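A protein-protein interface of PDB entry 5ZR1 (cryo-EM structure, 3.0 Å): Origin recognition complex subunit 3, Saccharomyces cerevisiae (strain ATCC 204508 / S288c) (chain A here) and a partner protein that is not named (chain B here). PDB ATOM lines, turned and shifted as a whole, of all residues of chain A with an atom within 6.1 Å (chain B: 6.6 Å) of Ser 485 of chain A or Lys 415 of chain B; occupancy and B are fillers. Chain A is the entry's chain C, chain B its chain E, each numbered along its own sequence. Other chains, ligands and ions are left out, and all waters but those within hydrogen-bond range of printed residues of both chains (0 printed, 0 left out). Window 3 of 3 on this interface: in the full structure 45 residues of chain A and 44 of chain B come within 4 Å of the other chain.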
ATOM      1  N   SER A 482       6.748 -13.939  21.333  1.00  0.00           N
ATOM      2  CA  SER A 482       7.003 -15.353  21.545  1.00  0.00           C
ATOM      3  C   SER A 482       5.703 -16.080  21.260  1.00  0.00           C
ATOM      4  O   SER A 482       4.856 -16.198  22.148  1.00  0.00           O
ATOM      5  CB  SER A 482       7.487 -15.621  22.969  1.00  0.00           C
ATOM      6  OG  SER A 482       8.733 -14.994  23.212  1.00  0.00           O
ATOM      7  N   TYR A 483       5.537 -16.541  20.017  1.00  0.00           N
ATOM      8  CA  TYR A 483       4.248 -17.033  19.535  1.00  0.00           C
ATOM      9  C   TYR A 483       3.820 -18.290  20.277  1.00  0.00           C
ATOM     10  O   TYR A 483       2.777 -18.308  20.935  1.00  0.00           O
ATOM     11  CB  TYR A 483       4.333 -17.330  18.041  1.00  0.00           C
ATOM     12  CG  TYR A 483       3.018 -17.706  17.394  1.00  0.00           C
ATOM     13  CD1 TYR A 483       2.165 -16.730  16.915  1.00  0.00           C
ATOM     14  CD2 TYR A 483       2.625 -19.037  17.272  1.00  0.00           C
ATOM     15  CE1 TYR A 483       0.982 -17.064  16.314  1.00  0.00           C
ATOM     16  CE2 TYR A 483       1.433 -19.376  16.687  1.00  0.00           C
ATOM     17  CZ  TYR A 483       0.616 -18.390  16.210  1.00  0.00           C
ATOM     18  OH  TYR A 483      -0.572 -18.737  15.622  1.00  0.00           O
ATOM     19  N   LYS A 484       4.615 -19.356  20.164  1.00  0.00           N
ATOM     20  CA  LYS A 484       4.234 -20.629  20.747  1.00  0.00           C
ATOM     21  C   LYS A 484       4.304 -20.594  22.263  1.00  0.00           C
ATOM     22  O   LYS A 484       3.487 -21.239  22.926  1.00  0.00           O
ATOM     23  CB  LYS A 484       5.095 -21.759  20.172  1.00  0.00           C
ATOM     24  CG  LYS A 484       6.576 -21.719  20.470  1.00  0.00           C
ATOM     25  CD  LYS A 484       7.292 -22.861  19.763  1.00  0.00           C
ATOM     26  CE  LYS A 484       6.949 -24.203  20.377  1.00  0.00           C
ATOM     27  NZ  LYS A 484       7.490 -24.311  21.755  1.00  0.00           N
ATOM     28  N   SER A 485       5.208 -19.794  22.823  1.00  0.00           N
ATOM     29  CA  SER A 485       5.301 -19.675  24.272  1.00  0.00           C
ATOM     30  C   SER A 485       4.099 -18.949  24.853  1.00  0.00           C
ATOM     31  O   SER A 485       3.727 -19.199  26.000  1.00  0.00           O
ATOM     32  CB  SER A 485       6.594 -18.964  24.651  1.00  0.00           C
ATOM     33  OG  SER A 485       7.713 -19.730  24.243  1.00  0.00           O
ATOM     34  N   ASN A 486       3.471 -18.063  24.080  1.00  0.00           N
ATOM     35  CA  ASN A 486       2.204 -17.490  24.507  1.00  0.00           C
ATOM     36  C   ASN A 486       1.054 -18.471  24.371  1.00  0.00           C
ATOM     37  O   ASN A 486       0.004 -18.255  24.976  1.00  0.00           O
ATOM     38  CB  ASN A 486       1.886 -16.227  23.715  1.00  0.00           C
ATOM     39  CG  ASN A 486       2.750 -15.062  24.118  1.00  0.00           C
ATOM     40  OD1 ASN A 486       3.047 -14.879  25.295  1.00  0.00           O
ATOM     41  ND2 ASN A 486       3.147 -14.255  23.147  1.00  0.00           N
ATOM     42  N   ILE A 487       1.216 -19.532  23.583  1.00  0.00           N
ATOM     43  CA  ILE A 487       0.160 -20.530  23.481  1.00  0.00           C
ATOM     44  C   ILE A 487       0.233 -21.507  24.646  1.00  0.00           C
ATOM     45  O   ILE A 487      -0.791 -21.833  25.258  1.00  0.00           O
ATOM     46  CB  ILE A 487       0.226 -21.261  22.128  1.00  0.00           C
ATOM     47  CG1 ILE A 487       0.153 -20.271  20.967  1.00  0.00           C
ATOM     48  CG2 ILE A 487      -0.908 -22.260  22.009  1.00  0.00           C
ATOM     49  CD1 ILE A 487      -1.107 -19.476  20.909  1.00  0.00           C
ATOM     50  N   GLU A 488       1.437 -21.987  24.987  1.00  0.00           N
ATOM     51  CA  GLU A 488       1.524 -22.963  26.070  1.00  0.00           C
ATOM     52  C   GLU A 488       1.334 -22.318  27.430  1.00  0.00           C
ATOM     53  O   GLU A 488       0.926 -22.998  28.372  1.00  0.00           O
ATOM     54  CB  GLU A 488       2.852 -23.719  26.082  1.00  0.00           C
ATOM     55  CG  GLU A 488       3.191 -24.521  24.852  1.00  0.00           C
ATOM     56  CD  GLU A 488       4.333 -23.914  24.087  1.00  0.00           C
ATOM     57  OE1 GLU A 488       4.992 -23.007  24.636  1.00  0.00           O
ATOM     58  OE2 GLU A 488       4.573 -24.318  22.937  1.00  0.00           O
ATOM     59  N   ASP A 489       1.628 -21.025  27.564  1.00  0.00           N
ATOM     60  CA  ASP A 489       1.373 -20.363  28.837  1.00  0.00           C
ATOM     61  C   ASP A 489      -0.117 -20.167  29.067  1.00  0.00           C
ATOM     62  O   ASP A 489      -0.588 -20.257  30.202  1.00  0.00           O
ATOM     63  CB  ASP A 489       2.097 -19.021  28.905  1.00  0.00           C
ATOM     64  CG  ASP A 489       3.592 -19.173  29.086  1.00  0.00           C
ATOM     65  OD1 ASP A 489       4.022 -20.203  29.644  1.00  0.00           O
ATOM     66  OD2 ASP A 489       4.338 -18.253  28.685  1.00  0.00           O
ATOM     67  N   ASN A 490      -0.878 -19.901  28.006  1.00  0.00           N
ATOM     68  CA  ASN A 490      -2.322 -19.781  28.161  1.00  0.00           C
ATOM     69  C   ASN A 490      -2.971 -21.137  28.380  1.00  0.00           C
ATOM     70  O   ASN A 490      -3.967 -21.233  29.103  1.00  0.00           O
ATOM     71  CB  ASN A 490      -2.936 -19.106  26.941  1.00  0.00           C
ATOM     72  CG  ASN A 490      -2.462 -17.692  26.769  1.00  0.00           C
ATOM     73  OD1 ASN A 490      -2.209 -16.993  27.738  1.00  0.00           O
ATOM     74  ND2 ASN A 490      -2.354 -17.255  25.525  1.00  0.00           N
ATOM     75  N   GLY A 615       8.379 -24.061  26.789  1.00  0.00           N
ATOM     76  CA  GLY A 615       9.691 -23.509  27.073  1.00  0.00           C
ATOM     77  C   GLY A 615      10.654 -23.489  25.904  1.00  0.00           C
ATOM     78  O   GLY A 615      11.527 -22.619  25.833  1.00  0.00           O
ATOM     79  N   ILE A 616      10.520 -24.444  24.991  1.00  0.00           N
ATOM     80  CA  ILE A 616      11.333 -24.467  23.790  1.00  0.00           C
ATOM     81  C   ILE A 616      10.881 -23.360  22.849  1.00  0.00           C
ATOM     82  O   ILE A 616      11.684 -22.556  22.374  1.00  0.00           O
ATOM     83  CB  ILE A 616      11.265 -25.831  23.102  1.00  0.00           C
ATOM     84  CG1 ILE A 616      11.854 -26.908  24.002  1.00  0.00           C
ATOM     85  CG2 ILE A 616      12.022 -25.805  21.820  1.00  0.00           C
ATOM     86  CD1 ILE A 616      11.690 -28.295  23.462  1.00  0.00           C
ATOM     87  OXT ILE A 616       9.692 -23.231  22.555  1.00  0.00           O
ATOM     88  N   PHE B 390      18.618 -25.997  19.037  1.00  0.00           N
ATOM     89  CA  PHE B 390      18.867 -24.570  18.828  1.00  0.00           C
ATOM     90  C   PHE B 390      19.071 -23.832  20.143  1.00  0.00           C
ATOM     91  O   PHE B 390      20.046 -23.093  20.300  1.00  0.00           O
ATOM     92  CB  PHE B 390      17.724 -23.933  18.040  1.00  0.00           C
ATOM     93  CG  PHE B 390      17.821 -22.443  17.936  1.00  0.00           C
ATOM     94  CD1 PHE B 390      18.780 -21.853  17.135  1.00  0.00           C
ATOM     95  CD2 PHE B 390      16.938 -21.632  18.628  1.00  0.00           C
ATOM     96  CE1 PHE B 390      18.866 -20.481  17.045  1.00  0.00           C
ATOM     97  CE2 PHE B 390      17.020 -20.264  18.538  1.00  0.00           C
ATOM     98  CZ  PHE B 390      17.983 -19.688  17.746  1.00  0.00           C
ATOM     99  N   GLN B 391      18.176 -24.023  21.110  1.00  0.00           N
ATOM    100  CA  GLN B 391      18.388 -23.320  22.367  1.00  0.00           C
ATOM    101  C   GLN B 391      19.381 -24.025  23.276  1.00  0.00           C
ATOM    102  O   GLN B 391      19.754 -23.461  24.307  1.00  0.00           O
ATOM    103  CB  GLN B 391      17.077 -23.100  23.118  1.00  0.00           C
ATOM    104  CG  GLN B 391      16.412 -24.339  23.624  1.00  0.00           C
ATOM    105  CD  GLN B 391      15.244 -24.017  24.528  1.00  0.00           C
ATOM    106  OE1 GLN B 391      15.000 -22.862  24.859  1.00  0.00           O
ATOM    107  NE2 GLN B 391      14.522 -25.038  24.940  1.00  0.00           N
ATOM    108  N   GLU B 410      14.297 -12.860  34.145  1.00  0.00           N
ATOM    109  CA  GLU B 410      15.204 -12.725  33.003  1.00  0.00           C
ATOM    110  C   GLU B 410      14.915 -13.750  31.899  1.00  0.00           C
ATOM    111  O   GLU B 410      14.886 -13.377  30.720  1.00  0.00           O
ATOM    112  CB  GLU B 410      16.668 -12.782  33.459  1.00  0.00           C
ATOM    113  CG  GLU B 410      17.181 -14.105  34.024  1.00  0.00           C
ATOM    114  CD  GLU B 410      18.632 -14.041  34.443  1.00  0.00           C
ATOM    115  OE1 GLU B 410      19.222 -12.944  34.372  1.00  0.00           O
ATOM    116  OE2 GLU B 410      19.190 -15.090  34.823  1.00  0.00           O
ATOM    117  N   GLU B 411      14.607 -15.002  32.264  1.00  0.00           N
ATOM    118  CA  GLU B 411      14.531 -16.151  31.350  1.00  0.00           C
ATOM    119  C   GLU B 411      15.744 -16.197  30.418  1.00  0.00           C
ATOM    120  O   GLU B 411      15.654 -15.926  29.221  1.00  0.00           O
ATOM    121  CB  GLU B 411      13.235 -16.192  30.532  1.00  0.00           C
ATOM    122  CG  GLU B 411      11.990 -16.494  31.340  1.00  0.00           C
ATOM    123  CD  GLU B 411      11.185 -15.260  31.650  1.00  0.00           C
ATOM    124  OE1 GLU B 411      11.440 -14.220  31.010  1.00  0.00           O
ATOM    125  OE2 GLU B 411      10.311 -15.326  32.538  1.00  0.00           O
ATOM    126  N   LEU B 413      17.483 -18.299  28.984  1.00  0.00           N
ATOM    127  CA  LEU B 413      17.528 -19.174  27.831  1.00  0.00           C
ATOM    128  C   LEU B 413      16.486 -18.743  26.805  1.00  0.00           C
ATOM    129  O   LEU B 413      15.389 -18.302  27.155  1.00  0.00           O
ATOM    130  CB  LEU B 413      17.302 -20.608  28.284  1.00  0.00           C
ATOM    131  CG  LEU B 413      17.615 -21.703  27.294  1.00  0.00           C
ATOM    132  CD1 LEU B 413      19.029 -21.517  26.817  1.00  0.00           C
ATOM    133  CD2 LEU B 413      17.537 -22.945  28.083  1.00  0.00           C
ATOM    134  N   MET B 414      16.843 -18.865  25.528  1.00  0.00           N
ATOM    135  CA  MET B 414      16.084 -18.238  24.454  1.00  0.00           C
ATOM    136  C   MET B 414      14.942 -19.124  23.976  1.00  0.00           C
ATOM    137  O   MET B 414      15.159 -20.274  23.585  1.00  0.00           O
ATOM    138  CB  MET B 414      16.986 -17.904  23.269  1.00  0.00           C
ATOM    139  CG  MET B 414      16.234 -17.172  22.174  1.00  0.00           C
ATOM    140  SD  MET B 414      17.216 -16.710  20.748  1.00  0.00           S
ATOM    141  CE  MET B 414      15.969 -15.963  19.712  1.00  0.00           C
ATOM    142  N   LYS B 415      13.736 -18.570  23.976  1.00  0.00           N
ATOM    143  CA  LYS B 415      12.561 -19.230  23.434  1.00  0.00           C
ATOM    144  C   LYS B 415      12.407 -18.908  21.949  1.00  0.00           C
ATOM    145  O   LYS B 415      13.080 -18.037  21.399  1.00  0.00           O
ATOM    146  CB  LYS B 415      11.319 -18.811  24.216  1.00  0.00           C
ATOM    147  CG  LYS B 415      11.345 -19.252  25.669  1.00  0.00           C
ATOM    148  CD  LYS B 415      10.091 -18.835  26.409  1.00  0.00           C
ATOM    149  CE  LYS B 415      10.074 -17.340  26.652  1.00  0.00           C
ATOM    150  NZ  LYS B 415      11.155 -16.926  27.585  1.00  0.00           N
ATOM    151  N   ALA B 416      11.500 -19.631  21.294  1.00  0.00           N
ATOM    152  CA  ALA B 416      11.275 -19.482  19.857  1.00  0.00           C
ATOM    153  C   ALA B 416      10.229 -18.399  19.636  1.00  0.00           C
ATOM    154  O   ALA B 416       9.026 -18.655  19.649  1.00  0.00           O
ATOM    155  CB  ALA B 416      10.842 -20.802  19.237  1.00  0.00           C
ATOM    156  N   ASN B 417      10.692 -17.173  19.409  1.00  0.00           N
ATOM    157  CA  ASN B 417       9.793 -16.068  19.107  1.00  0.00           C
ATOM    158  C   ASN B 417       9.438 -16.080  17.622  1.00  0.00           C
ATOM    159  O   ASN B 417       9.641 -17.070  16.916  1.00  0.00           O
ATOM    160  CB  ASN B 417      10.389 -14.739  19.572  1.00  0.00           C
ATOM    161  CG  ASN B 417      11.746 -14.441  18.969  1.00  0.00           C
ATOM    162  OD1 ASN B 417      12.287 -15.207  18.178  1.00  0.00           O
ATOM    163  ND2 ASN B 417      12.300 -13.295  19.339  1.00  0.00           N
ATOM    164  N   VAL B 420      12.554 -16.669  15.069  1.00  0.00           N
ATOM    165  CA  VAL B 420      13.158 -17.984  14.894  1.00  0.00           C
ATOM    166  C   VAL B 420      12.442 -18.751  13.791  1.00  0.00           C
ATOM    167  O   VAL B 420      13.079 -19.385  12.944  1.00  0.00           O
ATOM    168  CB  VAL B 420      13.144 -18.748  16.230  1.00  0.00           C
ATOM    169  CG1 VAL B 420      13.706 -20.144  16.064  1.00  0.00           C
ATOM    170  CG2 VAL B 420      13.926 -17.987  17.272  1.00  0.00           C
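N of Ala 416 of chain B sits at hydrogen-bond distance from O of Ile 616 of chain A (3.1 Å).
The side-chain amide oxygen (OE1) of Gln 391 of chain B sits close to the backbone carbonyl oxygen (O) of Met 414 of chain B, at 2.9 Å.
The backbone carbonyl oxygen of Ser 482 of chain A lies within hydrogen-bond range of the side-chain amide nitrogen of Asn 486 of chain A (2.8 Å).
The side-chain amide oxygen (OD1) of Asn 417 of chain B lies close to the backbone NH (N) of Val 420 of chain B, 3.4 Å away.
NZ of Lys 484 of chain A lies within salt-bridge range of OXT of Ile 616 of chain A, 2.6 Å away.
CA of Ser 482 of chain A touches CA of Asn 417 of chain B, at 3.8 Å.
OG of Ser 485 of chain A touches CD of Lys 415 of chain B, 3.3 Å away.
Gln 391 of chain B touches Gly 615 of chain A.
O of Gly 615 of chain A touches CG of Lys 415 of chain B (3.4 Å).
Gln 391 of chain B touches Ile 616 of chain A.
Ile 616 of chain A touches Lys 415 of chain B (O to CA, 3.6 Å).
Ser 485 of chain A touches just one residue of chain B: Lys 415 (3.3 Å).
Of chain A, only Ser 485 (3.3 Å), Gly 615 (3.4 Å) and Ile 616 (3.6 Å) come within 4 Å of Lys 415 of chain B.
Of the printed residues of chain A, Asn 417 of chain B touches Ser 482 (3.8 Å).
Printed residues of chain B within 4 Å of Gly 615 of chain A: Gln 391 and Lys 415.
The nearest residue of chain A that does not touch Lys 415 of chain B is Ser 482 of chain A (4.4 Å).
Of the 11 printed residues of chain A, 4 touch a printed residue of chain B.
Hydrophobic or aromatic side chains of chain B that line the printed part of chain A: Ala 416.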
